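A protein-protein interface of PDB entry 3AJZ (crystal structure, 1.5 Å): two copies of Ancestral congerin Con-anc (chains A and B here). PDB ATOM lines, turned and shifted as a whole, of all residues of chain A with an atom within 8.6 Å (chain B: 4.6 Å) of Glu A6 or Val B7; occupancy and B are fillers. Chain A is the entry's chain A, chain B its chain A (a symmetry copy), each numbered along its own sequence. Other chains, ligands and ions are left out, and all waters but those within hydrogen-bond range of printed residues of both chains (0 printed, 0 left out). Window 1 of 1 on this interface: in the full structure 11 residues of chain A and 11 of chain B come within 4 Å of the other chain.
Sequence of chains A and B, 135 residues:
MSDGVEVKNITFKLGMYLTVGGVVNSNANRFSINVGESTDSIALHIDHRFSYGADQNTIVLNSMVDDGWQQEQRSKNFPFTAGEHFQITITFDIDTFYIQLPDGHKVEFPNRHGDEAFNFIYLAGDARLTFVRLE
The backbone carbonyl oxygen of Gly A4 sits close to the side-chain amide oxygen of Asn B9. The backbone NH (N) of Lys B8 lies within hydrogen-bond range of the backbone carbonyl oxygen (O) of Glu A6 (2.8 Å). The backbone NH of Lys A8 is in hydrogen-bond range of the backbone carbonyl oxygen of Glu B6 (2.8 Å). The backbone carbonyl oxygen (O) of Val B132 is in hydrogen-bond range of the backbone NH (N) of Val A132, at 3.1 Å.
Val A5 touches Lys B8, and with the chains exchanged Lys A8 touches Val B5. Val A5 touches Asn B9, and with the chains exchanged Asn A9 touches Val B5. Glu B6 touches its own counterpart, Glu A6. Glu A6 touches Lys B8, and with the chains exchanged Lys A8 touches Glu B6. Positions printed for both chains: 5, 6, 7, 8, 9, 10, 119, 120, 121 and 132. Of the 15 pairs that touch across the chains among the printed residues, 13 have their exchanged pair printed and touching as well.
Hydrophobic or aromatic side chains of chain A that line the printed part of chain B: Val A5, Val A7, Phe A131 and Val A132. Among the printed residues, 15 pairs touch across the chains. Among the printed residues, no Asp or Glu carboxylate lies within 4 Å of a Lys or Arg side-chain nitrogen of the other chain.
Among the printed residues, pairs that only touch across the chains: Phe A131 with Val B132 (3.2 Å), Val A5 with Lys B8 (3.3 Å), Lys A8 with Val B5 (3.3 Å), Glu A6 with Val B7 (3.5 Å), Val A7 with Glu B6 (3.5 Å), Glu A6 with Glu B6 (3.6 Å), Asn A9 with Val B5 (3.6 Å), Val A5 with Asn B9 (3.6 Å), Val A5 with Val B7 (3.7 Å), Val A7 with Val B5 (3.7 Å) and Lys A8 with Lys B8 (3.8 Å).
Val B7 touches two residues of chain A. Printed residues of chain A within 4 Å of Lys B8: Val A5 (3.3 Å), Glu A6 (2.8 Å) and Lys A8 (3.8 Å). Of the printed residues of chain B, Phe A131 touches Val B132. Of the printed residues of chain B, Asn A9 touches Val B5 (3.6 Å). Printed residues of chain A within 4 Å of Val B5: Val A7, Lys A8 and Asn A9. Leu A123 touches none of the printed residues of chain B. Asn A119 touches none of the printed residues of chain B. The nearest printed residue of chain B that does not touch Glu A6 is Asn B9 (4.2 Å). The nearest printed residue of chain A that does not touch Lys B8 is Gly A4 (4.4 Å).
The backbone carbonyl oxygen of Val A5 lies within hydrogen-bond range of the backbone NH of Leu A123. The side-chain carboxylate (OE2) of Glu A6 lies within salt-bridge range of the side-chain amino group (NZ) of Lys A8 (2.8 Å). N of Asn A9 is in hydrogen-bond range of O of Asn A119. NZ of Lys B8 lies within salt-bridge range of OE2 of Glu B6 (2.8 Å). The backbone NH (N) of Val B7 sits at hydrogen-bond distance from the backbone carbonyl oxygen (O) of Ile B121 (2.8 Å). The backbone NH (N) of Asn B9 is in hydrogen-bond range of the backbone carbonyl oxygen (O) of Asn B119, at 2.9 Å.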
ATOM      1  N   GLY A   4       9.544 -13.931  19.424  1.00  0.00           N
ATOM      2  CA  GLY A   4       8.994 -14.548  20.671  1.00  0.00           C
ATOM      3  C   GLY A   4       8.876 -13.558  21.807  1.00  0.00           C
ATOM      4  O   GLY A   4       9.357 -12.409  21.703  1.00  0.00           O
ATOM      5  N   VAL A   5       8.211 -13.998  22.872  1.00  0.00           N
ATOM      6  CA  VAL A   5       7.940 -13.155  24.023  1.00  0.00           C
ATOM      7  C   VAL A   5       9.237 -12.669  24.636  1.00  0.00           C
ATOM      8  O   VAL A   5      10.156 -13.460  24.848  1.00  0.00           O
ATOM      9  CB  VAL A   5       7.086 -13.883  25.069  1.00  0.00           C
ATOM     10  CG1 VAL A   5       6.976 -13.074  26.330  1.00  0.00           C
ATOM     11  CG2 VAL A   5       5.701 -14.165  24.506  1.00  0.00           C
ATOM     12  N   GLU A   6       9.311 -11.370  24.913  1.00  0.00           N
ATOM     13  CA  GLU A   6      10.393 -10.820  25.719  1.00  0.00           C
ATOM     14  C   GLU A   6       9.862 -10.258  27.021  1.00  0.00           C
ATOM     15  O   GLU A   6       8.900  -9.504  27.016  1.00  0.00           O
ATOM     16  CB  GLU A   6      11.119  -9.703  24.998  1.00  0.00           C
ATOM     17  CG  GLU A   6      12.218  -9.136  25.888  1.00  0.00           C
ATOM     18  CD  GLU A   6      13.038  -8.052  25.238  1.00  0.00           C
ATOM     19  OE1 GLU A   6      14.167  -7.809  25.737  1.00  0.00           O
ATOM     20  OE2 GLU A   6      12.563  -7.441  24.246  1.00  0.00           O
ATOM     21  N   VAL A   7      10.508 -10.624  28.124  1.00  0.00           N
ATOM     22  CA  VAL A   7      10.168 -10.094  29.450  1.00  0.00           C
ATOM     23  C   VAL A   7      11.337  -9.207  29.838  1.00  0.00           C
ATOM     24  O   VAL A   7      12.451  -9.725  30.065  1.00  0.00           O
ATOM     25  CB  VAL A   7      10.004 -11.230  30.481  1.00  0.00           C
ATOM     26  CG1 VAL A   7       9.516 -10.687  31.838  1.00  0.00           C
ATOM     27  CG2 VAL A   7       9.051 -12.310  29.945  1.00  0.00           C
ATOM     28  N   LYS A   8      11.087  -7.897  29.929  1.00  0.00           N
ATOM     29  CA  LYS A   8      12.104  -6.847  30.112  1.00  0.00           C
ATOM     30  C   LYS A   8      11.946  -6.087  31.447  1.00  0.00           C
ATOM     31  O   LYS A   8      10.854  -6.067  32.021  1.00  0.00           O
ATOM     32  CB  LYS A   8      11.977  -5.882  28.925  1.00  0.00           C
ATOM     33  CG  LYS A   8      12.716  -4.558  29.016  1.00  0.00           C
ATOM     34  CD  LYS A   8      12.335  -3.625  27.852  1.00  0.00           C
ATOM     35  CE  LYS A   8      13.035  -3.993  26.548  1.00  0.00           C
ATOM     36  NZ  LYS A   8      12.372  -5.128  25.817  1.00  0.00           N
ATOM     37  N   ASN A   9      13.012  -5.419  31.902  1.00  0.00           N
ATOM     38  CA  ASN A   9      13.052  -4.664  33.166  1.00  0.00           C
ATOM     39  C   ASN A   9      12.797  -5.562  34.354  1.00  0.00           C
ATOM     40  O   ASN A   9      12.230  -5.120  35.362  1.00  0.00           O
ATOM     41  CB  ASN A   9      12.052  -3.491  33.248  1.00  0.00           C
ATOM     42  CG  ASN A   9      12.044  -2.619  32.033  1.00  0.00           C
ATOM     43  OD1 ASN A   9      10.972  -2.287  31.519  1.00  0.00           O
ATOM     44  ND2 ASN A   9      13.225  -2.225  31.564  1.00  0.00           N
ATOM     45  N   ILE A  10      13.183  -6.827  34.237  1.00  0.00           N
ATOM     46  CA  ILE A  10      13.151  -7.728  35.387  1.00  0.00           C
ATOM     47  C   ILE A  10      14.362  -7.429  36.283  1.00  0.00           C
ATOM     48  O   ILE A  10      15.329  -6.802  35.851  1.00  0.00           O
ATOM     49  CB  ILE A  10      13.067  -9.225  34.984  1.00  0.00           C
ATOM     50  CG1 ILE A  10      14.371  -9.694  34.328  1.00  0.00           C
ATOM     51  CG2 ILE A  10      11.923  -9.468  34.013  1.00  0.00           C
ATOM     52  CD1 ILE A  10      14.437 -11.186  34.095  1.00  0.00           C
ATOM     53  N   ASN A  34      16.801 -17.105  26.408  1.00  0.00           N
ATOM     54  CA  ASN A  34      17.906 -16.138  26.276  1.00  0.00           C
ATOM     55  C   ASN A  34      17.805 -15.169  27.418  1.00  0.00           C
ATOM     56  O   ASN A  34      16.839 -14.418  27.457  1.00  0.00           O
ATOM     57  CB  ASN A  34      17.764 -15.381  24.960  1.00  0.00           C
ATOM     58  CG  ASN A  34      17.835 -16.296  23.778  1.00  0.00           C
ATOM     59  OD1 ASN A  34      18.929 -16.590  23.296  1.00  0.00           O
ATOM     60  ND2 ASN A  34      16.695 -16.766  23.302  1.00  0.00           N
ATOM     61  N   GLY A  36      19.712 -12.051  29.770  1.00  0.00           N
ATOM     62  CA  GLY A  36      20.832 -11.127  29.659  1.00  0.00           C
ATOM     63  C   GLY A  36      20.596  -9.808  30.348  1.00  0.00           C
ATOM     64  O   GLY A  36      19.599  -9.615  31.070  1.00  0.00           O
ATOM     65  N   SER A  38      22.255  -6.608  28.844  1.00  0.00           N
ATOM     66  CA  SER A  38      22.513  -5.462  27.967  1.00  0.00           C
ATOM     67  C   SER A  38      22.073  -5.743  26.541  1.00  0.00           C
ATOM     68  O   SER A  38      21.979  -6.905  26.128  1.00  0.00           O
ATOM     69  CB  SER A  38      23.967  -4.982  28.060  1.00  0.00           C
ATOM     70  OG  SER A  38      24.848  -5.947  27.542  1.00  0.00           O
ATOM     71  N   THR A  39      21.806  -4.681  25.783  1.00  0.00           N
ATOM     72  CA  THR A  39      21.077  -4.805  24.514  1.00  0.00           C
ATOM     73  C   THR A  39      21.671  -5.671  23.383  1.00  0.00           C
ATOM     74  O   THR A  39      20.924  -6.325  22.658  1.00  0.00           O
ATOM     75  CB  THR A  39      20.660  -3.421  23.952  1.00  0.00           C
ATOM     76  OG1 THR A  39      21.830  -2.639  23.697  1.00  0.00           O
ATOM     77  CG2 THR A  39      19.776  -2.702  24.942  1.00  0.00           C
ATOM     78  N   SER A  41      23.793  -8.261  23.783  1.00  0.00           N
ATOM     79  CA  SER A  41      24.447  -9.376  24.445  1.00  0.00           C
ATOM     80  C   SER A  41      23.413 -10.330  25.004  1.00  0.00           C
ATOM     81  O   SER A  41      22.282  -9.943  25.247  1.00  0.00           O
ATOM     82  CB  SER A  41      25.377  -8.898  25.568  1.00  0.00           C
ATOM     83  OG  SER A  41      24.664  -8.309  26.646  1.00  0.00           O
ATOM     84  N   ASN A 119      18.348  -8.391  33.488  1.00  0.00           N
ATOM     85  CA  ASN A 119      17.156  -7.597  33.344  1.00  0.00           C
ATOM     86  C   ASN A 119      16.238  -7.996  32.196  1.00  0.00           C
ATOM     87  O   ASN A 119      15.210  -7.351  31.994  1.00  0.00           O
ATOM     88  CB  ASN A 119      17.532  -6.124  33.293  1.00  0.00           C
ATOM     89  CG  ASN A 119      18.453  -5.801  32.158  1.00  0.00           C
ATOM     90  OD1 ASN A 119      18.124  -6.014  30.985  1.00  0.00           O
ATOM     91  ND2 ASN A 119      19.632  -5.254  32.495  1.00  0.00           N
ATOM     92  N   PHE A 120      16.577  -9.066  31.475  1.00  0.00           N
ATOM     93  CA  PHE A 120      15.663  -9.596  30.451  1.00  0.00           C
ATOM     94  C   PHE A 120      15.762 -11.078  30.234  1.00  0.00           C
ATOM     95  O   PHE A 120      16.795 -11.694  30.498  1.00  0.00           O
ATOM     96  CB  PHE A 120      15.773  -8.879  29.102  1.00  0.00           C
ATOM     97  CG  PHE A 120      16.985  -9.258  28.296  1.00  0.00           C
ATOM     98  CD1 PHE A 120      18.080  -8.396  28.239  1.00  0.00           C
ATOM     99  CD2 PHE A 120      17.033 -10.465  27.596  1.00  0.00           C
ATOM    100  CE1 PHE A 120      19.219  -8.737  27.480  1.00  0.00           C
ATOM    101  CE2 PHE A 120      18.181 -10.837  26.858  1.00  0.00           C
ATOM    102  CZ  PHE A 120      19.264  -9.958  26.796  1.00  0.00           C
ATOM    103  N   ILE A 121      14.644 -11.641  29.781  1.00  0.00           N
ATOM    104  CA  ILE A 121      14.605 -13.021  29.285  1.00  0.00           C
ATOM    105  C   ILE A 121      13.685 -13.029  28.094  1.00  0.00           C
ATOM    106  O   ILE A 121      12.586 -12.454  28.146  1.00  0.00           O
ATOM    107  CB  ILE A 121      14.121 -14.103  30.354  1.00  0.00           C
ATOM    108  CG1 ILE A 121      14.071 -15.523  29.733  1.00  0.00           C
ATOM    109  CG2 ILE A 121      12.811 -13.667  31.065  1.00  0.00           C
ATOM    110  CD1 ILE A 121      12.760 -15.928  29.054  1.00  0.00           C
ATOM    111  N   TYR A 122      14.134 -13.649  26.999  1.00  0.00           N
ATOM    112  CA  TYR A 122      13.240 -13.846  25.864  1.00  0.00           C
ATOM    113  C   TYR A 122      13.338 -15.214  25.221  1.00  0.00           C
ATOM    114  O   TYR A 122      14.383 -15.894  25.304  1.00  0.00           O
ATOM    115  CB  TYR A 122      13.391 -12.741  24.809  1.00  0.00           C
ATOM    116  CG  TYR A 122      14.678 -12.759  24.024  1.00  0.00           C
ATOM    117  CD1 TYR A 122      14.790 -13.519  22.859  1.00  0.00           C
ATOM    118  CD2 TYR A 122      15.761 -11.981  24.421  1.00  0.00           C
ATOM    119  CE1 TYR A 122      15.978 -13.507  22.111  1.00  0.00           C
ATOM    120  CE2 TYR A 122      16.942 -11.950  23.696  1.00  0.00           C
ATOM    121  CZ  TYR A 122      17.051 -12.721  22.557  1.00  0.00           C
ATOM    122  OH  TYR A 122      18.217 -12.682  21.803  1.00  0.00           O
ATOM    123  N   LEU A 123      12.229 -15.644  24.624  1.00  0.00           N
ATOM    124  CA  LEU A 123      12.189 -16.921  23.919  1.00  0.00           C
ATOM    125  C   LEU A 123      12.364 -16.655  22.437  1.00  0.00           C
ATOM    126  O   LEU A 123      11.866 -15.656  21.953  1.00  0.00           O
ATOM    127  CB  LEU A 123      10.831 -17.620  24.156  1.00  0.00           C
ATOM    128  CG  LEU A 123      10.859 -19.146  24.145  1.00  0.00           C
ATOM    129  CD1 LEU A 123      11.582 -19.548  25.421  1.00  0.00           C
ATOM    130  CD2 LEU A 123       9.502 -19.756  24.180  1.00  0.00           C
ATOM    131  N   ALA A 124      13.052 -17.571  21.744  1.00  0.00           N
ATOM    132  CA  ALA A 124      13.148 -17.529  20.277  1.00  0.00           C
ATOM    133  C   ALA A 124      12.899 -18.900  19.678  1.00  0.00           C
ATOM    134  O   ALA A 124      13.104 -19.941  20.332  1.00  0.00           O
ATOM    135  CB  ALA A 124      14.526 -17.013  19.837  1.00  0.00           C
ATOM    136  N   LEU A 129       5.980 -19.177  24.753  1.00  0.00           N
ATOM    137  CA  LEU A 129       6.080 -19.012  26.193  1.00  0.00           C
ATOM    138  C   LEU A 129       4.666 -18.896  26.728  1.00  0.00           C
ATOM    139  O   LEU A 129       3.860 -18.142  26.177  1.00  0.00           O
ATOM    140  CB  LEU A 129       6.849 -17.727  26.494  1.00  0.00           C
ATOM    141  CG  LEU A 129       7.142 -17.316  27.945  1.00  0.00           C
ATOM    142  CD1 LEU A 129       8.484 -16.589  28.063  1.00  0.00           C
ATOM    143  CD2 LEU A 129       6.041 -16.433  28.529  1.00  0.00           C
ATOM    144  N   THR A 130       4.381 -19.655  27.785  1.00  0.00           N
ATOM    145  CA  THR A 130       3.079 -19.636  28.461  1.00  0.00           C
ATOM    146  C   THR A 130       3.169 -19.032  29.850  1.00  0.00           C
ATOM    147  O   THR A 130       2.167 -18.518  30.366  1.00  0.00           O
ATOM    148  CB  THR A 130       2.466 -21.042  28.591  1.00  0.00           C
ATOM    149  OG1 THR A 130       3.377 -21.933  29.232  1.00  0.00           O
ATOM    150  CG2 THR A 130       2.088 -21.597  27.208  1.00  0.00           C
ATOM    151  N   PHE A 131       4.338 -19.106  30.482  1.00  0.00           N
ATOM    152  CA  PHE A 131       4.454 -18.448  31.780  1.00  0.00           C
ATOM    153  C   PHE A 131       5.872 -18.156  32.168  1.00  0.00           C
ATOM    154  O   PHE A 131       6.819 -18.801  31.672  1.00  0.00           O
ATOM    155  CB  PHE A 131       3.700 -19.219  32.839  1.00  0.00           C
ATOM    156  CG  PHE A 131       4.446 -20.352  33.423  1.00  0.00           C
ATOM    157  CD1 PHE A 131       4.264 -21.653  32.923  1.00  0.00           C
ATOM    158  CD2 PHE A 131       5.273 -20.153  34.521  1.00  0.00           C
ATOM    159  CE1 PHE A 131       4.954 -22.751  33.483  1.00  0.00           C
ATOM    160  CE2 PHE A 131       5.966 -21.213  35.088  1.00  0.00           C
ATOM    161  CZ  PHE A 131       5.802 -22.518  34.585  1.00  0.00           C
ATOM    162  N   VAL A 132       6.002 -17.148  33.017  1.00  0.00           N
ATOM    163  CA  VAL A 132       7.284 -16.812  33.594  1.00  0.00           C
ATOM    164  C   VAL A 132       7.035 -16.510  35.050  1.00  0.00           C
ATOM    165  O   VAL A 132       6.047 -15.847  35.376  1.00  0.00           O
ATOM    166  CB  VAL A 132       7.948 -15.608  32.863  1.00  0.00           C
ATOM    167  CG1 VAL A 132       7.035 -14.436  32.735  1.00  0.00           C
ATOM    168  CG2 VAL A 132       9.221 -15.158  33.566  1.00  0.00           C
ATOM    169  N   VAL B   5       8.220  -4.269  35.093  1.00  0.00           N
ATOM    170  CA  VAL B   5       8.371  -5.339  34.123  1.00  0.00           C
ATOM    171  C   VAL B   5       7.453  -5.110  32.940  1.00  0.00           C
ATOM    172  O   VAL B   5       6.273  -4.812  33.121  1.00  0.00           O
ATOM    173  CB  VAL B   5       8.110  -6.714  34.752  1.00  0.00           C
ATOM    174  CG1 VAL B   5       8.081  -7.788  33.702  1.00  0.00           C
ATOM    175  CG2 VAL B   5       9.182  -7.024  35.787  1.00  0.00           C
ATOM    176  N   GLU B   6       7.998  -5.241  31.733  1.00  0.00           N
ATOM    177  CA  GLU B   6       7.182  -5.289  30.526  1.00  0.00           C
ATOM    178  C   GLU B   6       7.294  -6.640  29.854  1.00  0.00           C
ATOM    179  O   GLU B   6       8.394  -7.136  29.653  1.00  0.00           O
ATOM    180  CB  GLU B   6       7.605  -4.238  29.522  1.00  0.00           C
ATOM    181  CG  GLU B   6       6.750  -4.345  28.265  1.00  0.00           C
ATOM    182  CD  GLU B   6       7.057  -3.302  27.221  1.00  0.00           C
ATOM    183  OE1 GLU B   6       6.174  -3.082  26.354  1.00  0.00           O
ATOM    184  OE2 GLU B   6       8.168  -2.713  27.257  1.00  0.00           O
ATOM    185  N   VAL B   7       6.150  -7.217  29.502  1.00  0.00           N
ATOM    186  CA  VAL B   7       6.099  -8.484  28.763  1.00  0.00           C
ATOM    187  C   VAL B   7       5.592  -8.121  27.379  1.00  0.00           C
ATOM    188  O   VAL B   7       4.418  -7.716  27.242  1.00  0.00           O
ATOM    189  CB  VAL B   7       5.131  -9.483  29.432  1.00  0.00           C
ATOM    190  CG1 VAL B   7       5.178 -10.858  28.737  1.00  0.00           C
ATOM    191  CG2 VAL B   7       5.443  -9.612  30.931  1.00  0.00           C
ATOM    192  N   LYS B   8       6.454  -8.277  26.369  1.00  0.00           N
ATOM    193  CA  LYS B   8       6.235  -7.820  24.986  1.00  0.00           C
ATOM    194  C   LYS B   8       6.179  -8.984  23.972  1.00  0.00           C
ATOM    195  O   LYS B   8       6.709 -10.065  24.243  1.00  0.00           O
ATOM    196  CB  LYS B   8       7.382  -6.861  24.640  1.00  0.00           C
ATOM    197  CG  LYS B   8       7.553  -6.468  23.182  1.00  0.00           C
ATOM    198  CD  LYS B   8       8.852  -5.670  22.967  1.00  0.00           C
ATOM    199  CE  LYS B   8       8.728  -4.215  23.404  1.00  0.00           C
ATOM    200  NZ  LYS B   8       8.891  -4.023  24.888  1.00  0.00           N
ATOM    201  N   ASN B   9       5.595  -8.743  22.793  1.00  0.00           N
ATOM    202  CA  ASN B   9       5.427  -9.739  21.721  1.00  0.00           C
ATOM    203  C   ASN B   9       4.587 -10.908  22.179  1.00  0.00           C
ATOM    204  O   ASN B   9       4.788 -12.041  21.721  1.00  0.00           O
ATOM    205  CB  ASN B   9       6.747 -10.308  21.158  1.00  0.00           C
ATOM    206  CG  ASN B   9       7.771  -9.264  20.847  1.00  0.00           C
ATOM    207  OD1 ASN B   9       8.939  -9.415  21.217  1.00  0.00           O
ATOM    208  ND2 ASN B   9       7.361  -8.203  20.156  1.00  0.00           N
ATOM    209  N   ILE B  10       3.665 -10.653  23.101  1.00  0.00           N
ATOM    210  CA  ILE B  10       2.682 -11.666  23.476  1.00  0.00           C
ATOM    211  C   ILE B  10       1.597 -11.728  22.392  1.00  0.00           C
ATOM    212  O   ILE B  10       1.452 -10.806  21.590  1.00  0.00           O
ATOM    213  CB  ILE B  10       2.091 -11.444  24.894  1.00  0.00           C
ATOM    214  CG1 ILE B  10       1.199 -10.198  24.931  1.00  0.00           C
ATOM    215  CG2 ILE B  10       3.193 -11.281  25.929  1.00  0.00           C
ATOM    216  CD1 ILE B  10       0.429 -10.033  26.222  1.00  0.00           C
ATOM    217  N   ASN B 119      -0.520  -7.241  22.377  1.00  0.00           N
ATOM    218  CA  ASN B 119       0.826  -7.745  22.292  1.00  0.00           C
ATOM    219  C   ASN B 119       1.759  -7.316  23.415  1.00  0.00           C
ATOM    220  O   ASN B 119       2.932  -7.689  23.401  1.00  0.00           O
ATOM    221  CB  ASN B 119       1.397  -7.430  20.917  1.00  0.00           C
ATOM    222  CG  ASN B 119       1.426  -5.962  20.626  1.00  0.00           C
ATOM    223  OD1 ASN B 119       2.057  -5.178  21.344  1.00  0.00           O
ATOM    224  ND2 ASN B 119       0.747  -5.565  19.538  1.00  0.00           N
ATOM    225  N   PHE B 120       1.245  -6.576  24.400  1.00  0.00           N
ATOM    226  CA  PHE B 120       2.049  -6.254  25.588  1.00  0.00           C
ATOM    227  C   PHE B 120       1.255  -6.084  26.850  1.00  0.00           C
ATOM    228  O   PHE B 120       0.067  -5.760  26.819  1.00  0.00           O
ATOM    229  CB  PHE B 120       2.962  -5.039  25.399  1.00  0.00           C
ATOM    230  CG  PHE B 120       2.252  -3.715  25.452  1.00  0.00           C
ATOM    231  CD1 PHE B 120       1.980  -3.023  24.271  1.00  0.00           C
ATOM    232  CD2 PHE B 120       1.859  -3.159  26.671  1.00  0.00           C
ATOM    233  CE1 PHE B 120       1.321  -1.777  24.309  1.00  0.00           C
ATOM    234  CE2 PHE B 120       1.167  -1.927  26.724  1.00  0.00           C
ATOM    235  CZ  PHE B 120       0.916  -1.237  25.536  1.00  0.00           C
ATOM    236  N   ILE B 121       1.933  -6.351  27.965  1.00  0.00           N
ATOM    237  CA  ILE B 121       1.416  -6.021  29.297  1.00  0.00           C
ATOM    238  C   ILE B 121       2.587  -5.540  30.112  1.00  0.00           C
ATOM    239  O   ILE B 121       3.658  -6.166  30.100  1.00  0.00           O
ATOM    240  CB  ILE B 121       0.687  -7.226  30.049  1.00  0.00           C
ATOM    241  CG1 ILE B 121       0.211  -6.800  31.463  1.00  0.00           C
ATOM    242  CG2 ILE B 121       1.541  -8.523  30.025  1.00  0.00           C
ATOM    243  CD1 ILE B 121       1.212  -6.979  32.606  1.00  0.00           C
ATOM    244  N   VAL B 132       3.566 -14.068  35.262  1.00  0.00           N
ATOM    245  CA  VAL B 132       2.592 -13.824  34.223  1.00  0.00           C
ATOM    246  C   VAL B 132       2.293 -15.160  33.590  1.00  0.00           C
ATOM    247  O   VAL B 132       3.214 -15.949  33.364  1.00  0.00           O
ATOM    248  CB  VAL B 132       3.111 -12.796  33.175  1.00  0.00           C
ATOM    249  CG1 VAL B 132       4.462 -13.143  32.646  1.00  0.00           C
ATOM    250  CG2 VAL B 132       2.150 -12.656  32.003  1.00  0.00           C
